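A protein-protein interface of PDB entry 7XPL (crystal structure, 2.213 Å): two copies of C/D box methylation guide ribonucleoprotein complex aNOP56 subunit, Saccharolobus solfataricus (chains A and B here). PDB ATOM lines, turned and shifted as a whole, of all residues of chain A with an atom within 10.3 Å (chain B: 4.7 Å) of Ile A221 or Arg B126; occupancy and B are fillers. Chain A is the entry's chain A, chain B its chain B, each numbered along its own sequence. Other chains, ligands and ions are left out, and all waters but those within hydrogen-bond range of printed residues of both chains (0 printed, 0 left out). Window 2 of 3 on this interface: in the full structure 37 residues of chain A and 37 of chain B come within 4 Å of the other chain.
NH1 of Arg B130 lies within hydrogen-bond range of O of Ser A220 (2.9 Å). NH1 of Arg B130 lies within hydrogen-bond range of O of Gly A222 (2.9 Å).
The backbone NH of Ala A223 is in hydrogen-bond range of the backbone carbonyl oxygen of Ile A167 (2.9 Å). The side-chain hydroxyl (OG) of Ser A220 sits at hydrogen-bond distance from the side-chain carboxylate (OE2) of Glu A171 (3.0 Å). The guanidinium group (NH2) of Arg A192 is in hydrogen-bond range of the backbone carbonyl oxygen (O) of Gly A222. The backbone carbonyl oxygen (O) of Ala A223 lies within hydrogen-bond range of the guanidinium group (NH2) of Arg A192 (3.3 Å). The backbone NH (N) of Gly A222 is in hydrogen-bond range of the side-chain hydroxyl (OG) of Ser A220. The side-chain carboxylate of Glu B123 lies within salt-bridge range of the guanidinium group of Arg B126 (3.6 Å).
Among the printed residues, pairs that only touch across the chains: Ala A223 with Ala B133, Ile A221 with Arg B130, Ile A167 with Ala B133, Ile A221 with Leu B129 and Ile A221 with Arg B126.
Ile A221 touches just these residues of chain B: Arg B126 (3.9 Å), Leu B129 (3.6 Å) and Arg B130 (3.3 Å). Arg B126 touches one residue of chain A. Leu B122 touches none of the printed residues of chain A. No residue of chain A comes within 4 Å of Glu B123. Leu B129 touches just one residue of chain A: Ile A221 (3.6 Å). Arg B130 touches just these residues of chain A: Ser A220, Ile A221 and Gly A222. Of the printed residues of chain A, Ala B133 touches Ile A167 (3.6 Å) and Ala A223 (3.3 Å). Of the printed residues of chain B, Ser A220 touches Arg B130. Printed residues of chain B within 4 Å of Ile A167: Ala B133 (3.6 Å). Printed residues of chain B within 4 Å of Gly A222: Arg B130. Ala A216 touches none of the printed residues of chain B.
Printed residues of chain A that touch a printed residue of chain B: Ile A167, Ser A220, Ile A221, Gly A222 and Ala A223. Hydrophobic or aromatic side chains of chain B within 4 Å of the printed part of chain A: Leu B129 and Ala B133. Among the printed residues, 7 pairs touch across the chains. Among the printed residues, no Asp or Glu carboxylate lies within 4 Å of a Lys or Arg side-chain nitrogen of the other chain.
No position is printed for both chains. Of the 7 pairs that touch across the chains among the printed residues, none has its exchanged pair printed and touching as well.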
ATOM      1  N   TYR A 165       8.307   9.779  -7.989  1.00  0.00           N
ATOM      2  CA  TYR A 165       8.982  10.386  -9.124  1.00  0.00           C
ATOM      3  C   TYR A 165       8.065  11.327  -9.907  1.00  0.00           C
ATOM      4  O   TYR A 165       8.547  12.284 -10.523  1.00  0.00           O
ATOM      5  CB  TYR A 165       9.531   9.281 -10.024  1.00  0.00           C
ATOM      6  CG  TYR A 165      10.423   9.786 -11.118  1.00  0.00           C
ATOM      7  CD1 TYR A 165      11.696  10.269 -10.824  1.00  0.00           C
ATOM      8  CD2 TYR A 165      10.006   9.780 -12.445  1.00  0.00           C
ATOM      9  CE1 TYR A 165      12.527  10.737 -11.826  1.00  0.00           C
ATOM     10  CE2 TYR A 165      10.835  10.249 -13.464  1.00  0.00           C
ATOM     11  CZ  TYR A 165      12.093  10.728 -13.140  1.00  0.00           C
ATOM     12  OH  TYR A 165      12.938  11.207 -14.114  1.00  0.00           O
ATOM     13  N   SER A 166       6.749  11.099  -9.893  1.00  0.00           N
ATOM     14  CA  SER A 166       5.857  12.047 -10.560  1.00  0.00           C
ATOM     15  C   SER A 166       5.958  13.469 -10.005  1.00  0.00           C
ATOM     16  O   SER A 166       5.546  14.402 -10.693  1.00  0.00           O
ATOM     17  CB  SER A 166       4.393  11.588 -10.469  1.00  0.00           C
ATOM     18  OG  SER A 166       4.160  10.440 -11.287  1.00  0.00           O
ATOM     19  N   ILE A 167       6.444  13.663  -8.772  1.00  0.00           N
ATOM     20  CA  ILE A 167       6.649  15.027  -8.279  1.00  0.00           C
ATOM     21  C   ILE A 167       7.575  15.793  -9.217  1.00  0.00           C
ATOM     22  O   ILE A 167       7.357  16.975  -9.512  1.00  0.00           O
ATOM     23  CB  ILE A 167       7.205  15.019  -6.845  1.00  0.00           C
ATOM     24  CG1 ILE A 167       6.116  14.632  -5.843  1.00  0.00           C
ATOM     25  CG2 ILE A 167       7.798  16.419  -6.475  1.00  0.00           C
ATOM     26  CD1 ILE A 167       6.671  14.385  -4.394  1.00  0.00           C
ATOM     27  N   HIS A 168       8.609  15.121  -9.709  1.00  0.00           N
ATOM     28  CA  HIS A 168       9.603  15.696 -10.592  1.00  0.00           C
ATOM     29  C   HIS A 168       9.219  15.562 -12.062  1.00  0.00           C
ATOM     30  O   HIS A 168       9.443  16.491 -12.845  1.00  0.00           O
ATOM     31  CB  HIS A 168      10.955  15.028 -10.336  1.00  0.00           C
ATOM     32  CG  HIS A 168      11.999  15.372 -11.355  1.00  0.00           C
ATOM     33  ND1 HIS A 168      12.591  16.616 -11.426  1.00  0.00           N
ATOM     34  CD2 HIS A 168      12.562  14.635 -12.343  1.00  0.00           C
ATOM     35  CE1 HIS A 168      13.460  16.632 -12.419  1.00  0.00           C
ATOM     36  NE2 HIS A 168      13.467  15.442 -12.989  1.00  0.00           N
ATOM     37  N   PHE A 169       8.648  14.424 -12.475  1.00  0.00           N
ATOM     38  CA  PHE A 169       8.363  14.175 -13.887  1.00  0.00           C
ATOM     39  C   PHE A 169       6.990  13.515 -14.021  1.00  0.00           C
ATOM     40  O   PHE A 169       6.875  12.332 -14.353  1.00  0.00           O
ATOM     41  CB  PHE A 169       9.491  13.344 -14.516  1.00  0.00           C
ATOM     42  CG  PHE A 169       9.403  13.216 -16.025  1.00  0.00           C
ATOM     43  CD1 PHE A 169       8.427  13.880 -16.746  1.00  0.00           C
ATOM     44  CD2 PHE A 169      10.286  12.408 -16.711  1.00  0.00           C
ATOM     45  CE1 PHE A 169       8.339  13.729 -18.148  1.00  0.00           C
ATOM     46  CE2 PHE A 169      10.199  12.259 -18.092  1.00  0.00           C
ATOM     47  CZ  PHE A 169       9.227  12.923 -18.807  1.00  0.00           C
ATOM     48  N   PRO A 170       5.914  14.289 -13.820  1.00  0.00           N
ATOM     49  CA  PRO A 170       4.576  13.682 -13.699  1.00  0.00           C
ATOM     50  C   PRO A 170       4.047  13.072 -14.974  1.00  0.00           C
ATOM     51  O   PRO A 170       3.256  12.118 -14.901  1.00  0.00           O
ATOM     52  CB  PRO A 170       3.698  14.856 -13.243  1.00  0.00           C
ATOM     53  CG  PRO A 170       4.454  16.091 -13.658  1.00  0.00           C
ATOM     54  CD  PRO A 170       5.898  15.729 -13.509  1.00  0.00           C
ATOM     55  N   GLU A 171       4.449  13.577 -16.142  1.00  0.00           N
ATOM     56  CA  GLU A 171       3.900  13.064 -17.396  1.00  0.00           C
ATOM     57  C   GLU A 171       4.463  11.699 -17.742  1.00  0.00           C
ATOM     58  O   GLU A 171       3.882  11.001 -18.581  1.00  0.00           O
ATOM     59  CB  GLU A 171       4.166  14.039 -18.564  1.00  0.00           C
ATOM     60  CG  GLU A 171       3.773  15.506 -18.294  1.00  0.00           C
ATOM     61  CD  GLU A 171       4.778  16.300 -17.421  1.00  0.00           C
ATOM     62  OE1 GLU A 171       4.540  17.518 -17.161  1.00  0.00           O
ATOM     63  OE2 GLU A 171       5.798  15.717 -16.976  1.00  0.00           O
ATOM     64  N   LEU A 172       5.579  11.299 -17.118  1.00  0.00           N
ATOM     65  CA  LEU A 172       6.160  10.005 -17.452  1.00  0.00           C
ATOM     66  C   LEU A 172       5.244   8.855 -17.032  1.00  0.00           C
ATOM     67  O   LEU A 172       5.244   7.800 -17.674  1.00  0.00           O
ATOM     68  CB  LEU A 172       7.536   9.862 -16.807  1.00  0.00           C
ATOM     69  CG  LEU A 172       8.290   8.593 -17.221  1.00  0.00           C
ATOM     70  CD1 LEU A 172       8.667   8.660 -18.687  1.00  0.00           C
ATOM     71  CD2 LEU A 172       9.513   8.305 -16.369  1.00  0.00           C
ATOM     72  N   ARG A 192      15.167  14.169 -15.067  1.00  0.00           N
ATOM     73  CA  ARG A 192      14.672  14.021 -16.427  1.00  0.00           C
ATOM     74  C   ARG A 192      15.503  14.833 -17.418  1.00  0.00           C
ATOM     75  O   ARG A 192      15.384  14.625 -18.629  1.00  0.00           O
ATOM     76  CB  ARG A 192      13.211  14.456 -16.502  1.00  0.00           C
ATOM     77  CG  ARG A 192      13.072  15.951 -16.336  1.00  0.00           C
ATOM     78  CD  ARG A 192      11.655  16.426 -16.493  1.00  0.00           C
ATOM     79  NE  ARG A 192      11.263  17.158 -15.305  1.00  0.00           N
ATOM     80  CZ  ARG A 192      11.154  18.476 -15.222  1.00  0.00           C
ATOM     81  NH1 ARG A 192      11.386  19.242 -16.275  1.00  0.00           N
ATOM     82  NH2 ARG A 192      10.790  19.015 -14.067  1.00  0.00           N
ATOM     83  N   LEU A 214      11.106  12.509 -24.555  1.00  0.00           N
ATOM     84  CA  LEU A 214      11.921  13.721 -24.555  1.00  0.00           C
ATOM     85  C   LEU A 214      11.052  14.953 -24.678  1.00  0.00           C
ATOM     86  O   LEU A 214      11.270  15.944 -23.977  1.00  0.00           O
ATOM     87  CB  LEU A 214      12.949  13.684 -25.676  1.00  0.00           C
ATOM     88  CG  LEU A 214      13.958  12.558 -25.517  1.00  0.00           C
ATOM     89  CD1 LEU A 214      14.761  12.410 -26.787  1.00  0.00           C
ATOM     90  CD2 LEU A 214      14.859  12.794 -24.310  1.00  0.00           C
ATOM     91  N   ASP A 215      10.030  14.905 -25.523  1.00  0.00           N
ATOM     92  CA  ASP A 215       9.147  16.063 -25.596  1.00  0.00           C
ATOM     93  C   ASP A 215       8.494  16.341 -24.240  1.00  0.00           C
ATOM     94  O   ASP A 215       8.499  17.480 -23.760  1.00  0.00           O
ATOM     95  CB  ASP A 215       8.102  15.868 -26.683  1.00  0.00           C
ATOM     96  CG  ASP A 215       7.625  17.184 -27.243  1.00  0.00           C
ATOM     97  OD1 ASP A 215       6.577  17.683 -26.775  1.00  0.00           O
ATOM     98  OD2 ASP A 215       8.322  17.738 -28.128  1.00  0.00           O
ATOM     99  N   ALA A 216       7.969  15.301 -23.579  1.00  0.00           N
ATOM    100  CA  ALA A 216       7.307  15.500 -22.291  1.00  0.00           C
ATOM    101  C   ALA A 216       8.273  16.045 -21.251  1.00  0.00           C
ATOM    102  O   ALA A 216       7.892  16.874 -20.417  1.00  0.00           O
ATOM    103  CB  ALA A 216       6.678  14.193 -21.800  1.00  0.00           C
ATOM    104  N   ALA A 217       9.536  15.620 -21.306  1.00  0.00           N
ATOM    105  CA  ALA A 217      10.505  16.080 -20.316  1.00  0.00           C
ATOM    106  C   ALA A 217      10.833  17.556 -20.505  1.00  0.00           C
ATOM    107  O   ALA A 217      10.976  18.294 -19.516  1.00  0.00           O
ATOM    108  CB  ALA A 217      11.771  15.225 -20.382  1.00  0.00           C
ATOM    109  N   LYS A 218      10.950  18.007 -21.763  1.00  0.00           N
ATOM    110  CA  LYS A 218      11.144  19.432 -22.034  1.00  0.00           C
ATOM    111  C   LYS A 218      10.014  20.263 -21.438  1.00  0.00           C
ATOM    112  O   LYS A 218      10.250  21.229 -20.704  1.00  0.00           O
ATOM    113  CB  LYS A 218      11.225  19.692 -23.545  1.00  0.00           C
ATOM    114  CG  LYS A 218      12.259  18.879 -24.311  1.00  0.00           C
ATOM    115  CD  LYS A 218      12.334  19.335 -25.776  1.00  0.00           C
ATOM    116  CE  LYS A 218      13.388  18.550 -26.577  1.00  0.00           C
ATOM    117  NZ  LYS A 218      12.918  17.196 -26.991  1.00  0.00           N
ATOM    118  N   LYS A 219       8.769  19.892 -21.738  1.00  0.00           N
ATOM    119  CA  LYS A 219       7.624  20.698 -21.331  1.00  0.00           C
ATOM    120  C   LYS A 219       7.111  20.354 -19.932  1.00  0.00           C
ATOM    121  O   LYS A 219       6.067  20.877 -19.528  1.00  0.00           O
ATOM    122  CB  LYS A 219       6.473  20.559 -22.341  1.00  0.00           C
ATOM    123  CG  LYS A 219       6.845  20.047 -23.733  1.00  0.00           C
ATOM    124  CD  LYS A 219       7.859  20.928 -24.460  1.00  0.00           C
ATOM    125  CE  LYS A 219       8.326  20.258 -25.768  1.00  0.00           C
ATOM    126  NZ  LYS A 219       9.447  20.992 -26.448  1.00  0.00           N
ATOM    127  N   SER A 220       7.817  19.519 -19.179  1.00  0.00           N
ATOM    128  CA  SER A 220       7.255  19.005 -17.941  1.00  0.00           C
ATOM    129  C   SER A 220       6.988  20.131 -16.954  1.00  0.00           C
ATOM    130  O   SER A 220       7.797  21.045 -16.788  1.00  0.00           O
ATOM    131  CB  SER A 220       8.201  17.990 -17.305  1.00  0.00           C
ATOM    132  OG  SER A 220       7.789  17.708 -15.975  1.00  0.00           O
ATOM    133  N   ILE A 221       5.852  20.046 -16.273  1.00  0.00           N
ATOM    134  CA  ILE A 221       5.554  20.962 -15.194  1.00  0.00           C
ATOM    135  C   ILE A 221       5.933  20.371 -13.838  1.00  0.00           C
ATOM    136  O   ILE A 221       5.505  20.874 -12.803  1.00  0.00           O
ATOM    137  CB  ILE A 221       4.087  21.402 -15.218  1.00  0.00           C
ATOM    138  CG1 ILE A 221       3.168  20.187 -15.199  1.00  0.00           C
ATOM    139  CG2 ILE A 221       3.817  22.272 -16.438  1.00  0.00           C
ATOM    140  CD1 ILE A 221       1.744  20.594 -15.013  1.00  0.00           C
ATOM    141  N   GLY A 222       6.753  19.333 -13.829  1.00  0.00           N
ATOM    142  CA  GLY A 222       7.216  18.781 -12.576  1.00  0.00           C
ATOM    143  C   GLY A 222       8.166  19.718 -11.865  1.00  0.00           C
ATOM    144  O   GLY A 222       8.695  20.676 -12.422  1.00  0.00           O
ATOM    145  N   ALA A 223       8.386  19.433 -10.593  1.00  0.00           N
ATOM    146  CA  ALA A 223       9.235  20.295  -9.801  1.00  0.00           C
ATOM    147  C   ALA A 223      10.696  20.042 -10.141  1.00  0.00           C
ATOM    148  O   ALA A 223      11.050  19.022 -10.739  1.00  0.00           O
ATOM    149  CB  ALA A 223       8.997  20.063  -8.305  1.00  0.00           C
ATOM    150  N   ASP A 224      11.543  21.002  -9.771  1.00  0.00           N
ATOM    151  CA  ASP A 224      12.985  20.812  -9.738  1.00  0.00           C
ATOM    152  C   ASP A 224      13.372  20.441  -8.319  1.00  0.00           C
ATOM    153  O   ASP A 224      12.922  21.081  -7.361  1.00  0.00           O
ATOM    154  CB  ASP A 224      13.738  22.068 -10.193  1.00  0.00           C
ATOM    155  CG  ASP A 224      13.599  22.316 -11.682  1.00  0.00           C
ATOM    156  OD1 ASP A 224      13.191  21.369 -12.416  1.00  0.00           O
ATOM    157  OD2 ASP A 224      13.892  23.457 -12.110  1.00  0.00           O
ATOM    158  N   ILE A 225      14.180  19.389  -8.191  1.00  0.00           N
ATOM    159  CA  ILE A 225      14.535  18.813  -6.904  1.00  0.00           C
ATOM    160  C   ILE A 225      16.026  18.499  -6.922  1.00  0.00           C
ATOM    161  O   ILE A 225      16.634  18.335  -7.982  1.00  0.00           O
ATOM    162  CB  ILE A 225      13.722  17.514  -6.592  1.00  0.00           C
ATOM    163  CG1 ILE A 225      14.190  16.365  -7.465  1.00  0.00           C
ATOM    164  CG2 ILE A 225      12.215  17.702  -6.807  1.00  0.00           C
ATOM    165  CD1 ILE A 225      13.629  15.033  -7.009  1.00  0.00           C
ATOM    166  N   LEU B 122      -5.268  26.990 -19.287  1.00  0.00           N
ATOM    167  CA  LEU B 122      -4.239  25.957 -19.280  1.00  0.00           C
ATOM    168  C   LEU B 122      -2.963  26.464 -18.628  1.00  0.00           C
ATOM    169  O   LEU B 122      -2.380  25.789 -17.771  1.00  0.00           O
ATOM    170  CB  LEU B 122      -3.955  25.472 -20.700  1.00  0.00           C
ATOM    171  CG  LEU B 122      -5.085  24.774 -21.459  1.00  0.00           C
ATOM    172  CD1 LEU B 122      -4.601  24.246 -22.821  1.00  0.00           C
ATOM    173  CD2 LEU B 122      -5.705  23.657 -20.616  1.00  0.00           C
ATOM    174  N   GLU B 123      -2.533  27.672 -18.999  1.00  0.00           N
ATOM    175  CA  GLU B 123      -1.290  28.215 -18.472  1.00  0.00           C
ATOM    176  C   GLU B 123      -1.406  28.525 -16.979  1.00  0.00           C
ATOM    177  O   GLU B 123      -0.509  28.206 -16.187  1.00  0.00           O
ATOM    178  CB  GLU B 123      -0.916  29.462 -19.276  1.00  0.00           C
ATOM    179  CG  GLU B 123       0.411  30.065 -18.903  1.00  0.00           C
ATOM    180  CD  GLU B 123       1.570  29.062 -18.892  1.00  0.00           C
ATOM    181  OE1 GLU B 123       1.498  28.005 -19.567  1.00  0.00           O
ATOM    182  OE2 GLU B 123       2.560  29.342 -18.173  1.00  0.00           O
ATOM    183  N   TYR B 124      -2.496  29.176 -16.585  1.00  0.00           N
ATOM    184  CA  TYR B 124      -2.762  29.399 -15.179  1.00  0.00           C
ATOM    185  C   TYR B 124      -2.696  28.084 -14.397  1.00  0.00           C
ATOM    186  O   TYR B 124      -2.008  27.982 -13.373  1.00  0.00           O
ATOM    187  CB  TYR B 124      -4.128  30.067 -15.055  1.00  0.00           C
ATOM    188  CG  TYR B 124      -4.510  30.482 -13.682  1.00  0.00           C
ATOM    189  CD1 TYR B 124      -3.736  31.381 -12.978  1.00  0.00           C
ATOM    190  CD2 TYR B 124      -5.655  29.973 -13.080  1.00  0.00           C
ATOM    191  CE1 TYR B 124      -4.081  31.782 -11.718  1.00  0.00           C
ATOM    192  CE2 TYR B 124      -6.016  30.359 -11.802  1.00  0.00           C
ATOM    193  CZ  TYR B 124      -5.221  31.276 -11.134  1.00  0.00           C
ATOM    194  OH  TYR B 124      -5.551  31.682  -9.863  1.00  0.00           O
ATOM    195  N   THR B 125      -3.361  27.049 -14.910  1.00  0.00           N
ATOM    196  CA  THR B 125      -3.394  25.786 -14.201  1.00  0.00           C
ATOM    197  C   THR B 125      -2.016  25.135 -14.155  1.00  0.00           C
ATOM    198  O   THR B 125      -1.591  24.674 -13.095  1.00  0.00           O
ATOM    199  CB  THR B 125      -4.422  24.842 -14.834  1.00  0.00           C
ATOM    200  OG1 THR B 125      -5.738  25.361 -14.620  1.00  0.00           O
ATOM    201  CG2 THR B 125      -4.326  23.461 -14.183  1.00  0.00           C
ATOM    202  N   ARG B 126      -1.305  25.082 -15.288  1.00  0.00           N
ATOM    203  CA  ARG B 126       0.054  24.531 -15.276  1.00  0.00           C
ATOM    204  C   ARG B 126       0.926  25.192 -14.209  1.00  0.00           C
ATOM    205  O   ARG B 126       1.697  24.506 -13.521  1.00  0.00           O
ATOM    206  CB  ARG B 126       0.727  24.675 -16.645  1.00  0.00           C
ATOM    207  CG  ARG B 126       0.093  23.874 -17.746  1.00  0.00           C
ATOM    208  CD  ARG B 126       0.977  23.846 -18.993  1.00  0.00           C
ATOM    209  NE  ARG B 126       0.264  23.247 -20.122  1.00  0.00           N
ATOM    210  CZ  ARG B 126      -0.294  23.938 -21.119  1.00  0.00           C
ATOM    211  NH1 ARG B 126      -0.209  25.271 -21.136  1.00  0.00           N
ATOM    212  NH2 ARG B 126      -0.933  23.298 -22.097  1.00  0.00           N
ATOM    213  N   ARG B 127       0.792  26.514 -14.029  1.00  0.00           N
ATOM    214  CA  ARG B 127       1.625  27.216 -13.052  1.00  0.00           C
ATOM    215  C   ARG B 127       1.225  26.869 -11.624  1.00  0.00           C
ATOM    216  O   ARG B 127       2.093  26.689 -10.760  1.00  0.00           O
ATOM    217  CB  ARG B 127       1.558  28.728 -13.265  1.00  0.00           C
ATOM    218  CG  ARG B 127       2.340  29.205 -14.487  1.00  0.00           C
ATOM    219  CD  ARG B 127       3.084  30.505 -14.189  1.00  0.00           C
ATOM    220  NE  ARG B 127       3.682  30.473 -12.846  1.00  0.00           N
ATOM    221  CZ  ARG B 127       4.297  31.502 -12.256  1.00  0.00           C
ATOM    222  NH1 ARG B 127       4.794  31.362 -11.023  1.00  0.00           N
ATOM    223  NH2 ARG B 127       4.404  32.666 -12.892  1.00  0.00           N
ATOM    224  N   LYS B 128      -0.075  26.770 -11.354  1.00  0.00           N
ATOM    225  CA  LYS B 128      -0.493  26.370 -10.016  1.00  0.00           C
ATOM    226  C   LYS B 128      -0.130  24.915  -9.729  1.00  0.00           C
ATOM    227  O   LYS B 128       0.166  24.584  -8.580  1.00  0.00           O
ATOM    228  CB  LYS B 128      -1.991  26.632  -9.827  1.00  0.00           C
ATOM    229  CG  LYS B 128      -2.338  28.140  -9.892  1.00  0.00           C
ATOM    230  CD  LYS B 128      -3.661  28.492  -9.239  1.00  0.00           C
ATOM    231  CE  LYS B 128      -3.486  28.656  -7.729  1.00  0.00           C
ATOM    232  NZ  LYS B 128      -4.735  28.283  -6.963  1.00  0.00           N
ATOM    233  N   LEU B 129      -0.090  24.053 -10.754  1.00  0.00           N
ATOM    234  CA  LEU B 129       0.401  22.684 -10.578  1.00  0.00           C
ATOM    235  C   LEU B 129       1.900  22.649 -10.282  1.00  0.00           C
ATOM    236  O   LEU B 129       2.357  21.910  -9.400  1.00  0.00           O
ATOM    237  CB  LEU B 129       0.104  21.861 -11.831  1.00  0.00           C
ATOM    238  CG  LEU B 129      -1.345  21.414 -12.066  1.00  0.00           C
ATOM    239  CD1 LEU B 129      -1.510  20.738 -13.422  1.00  0.00           C
ATOM    240  CD2 LEU B 129      -1.783  20.462 -10.949  1.00  0.00           C
ATOM    241  N   ARG B 130       2.688  23.429 -11.019  1.00  0.00           N
ATOM    242  CA  ARG B 130       4.118  23.508 -10.732  1.00  0.00           C
ATOM    243  C   ARG B 130       4.375  23.971  -9.300  1.00  0.00           C
ATOM    244  O   ARG B 130       5.195  23.382  -8.588  1.00  0.00           O
ATOM    245  CB  ARG B 130       4.806  24.457 -11.712  1.00  0.00           C
ATOM    246  CG  ARG B 130       6.264  24.743 -11.345  1.00  0.00           C
ATOM    247  CD  ARG B 130       7.195  23.932 -12.228  1.00  0.00           C
ATOM    248  NE  ARG B 130       6.966  24.260 -13.639  1.00  0.00           N
ATOM    249  CZ  ARG B 130       7.528  23.637 -14.674  1.00  0.00           C
ATOM    250  NH1 ARG B 130       8.371  22.621 -14.482  1.00  0.00           N
ATOM    251  NH2 ARG B 130       7.236  24.032 -15.913  1.00  0.00           N
ATOM    252  N   ALA B 133       3.714  21.300  -6.807  1.00  0.00           N
ATOM    253  CA  ALA B 133       4.724  20.248  -6.856  1.00  0.00           C
ATOM    254  C   ALA B 133       6.035  20.668  -6.202  1.00  0.00           C
ATOM    255  O   ALA B 133       6.822  19.797  -5.832  1.00  0.00           O
ATOM    256  CB  ALA B 133       4.981  19.815  -8.299  1.00  0.00           C
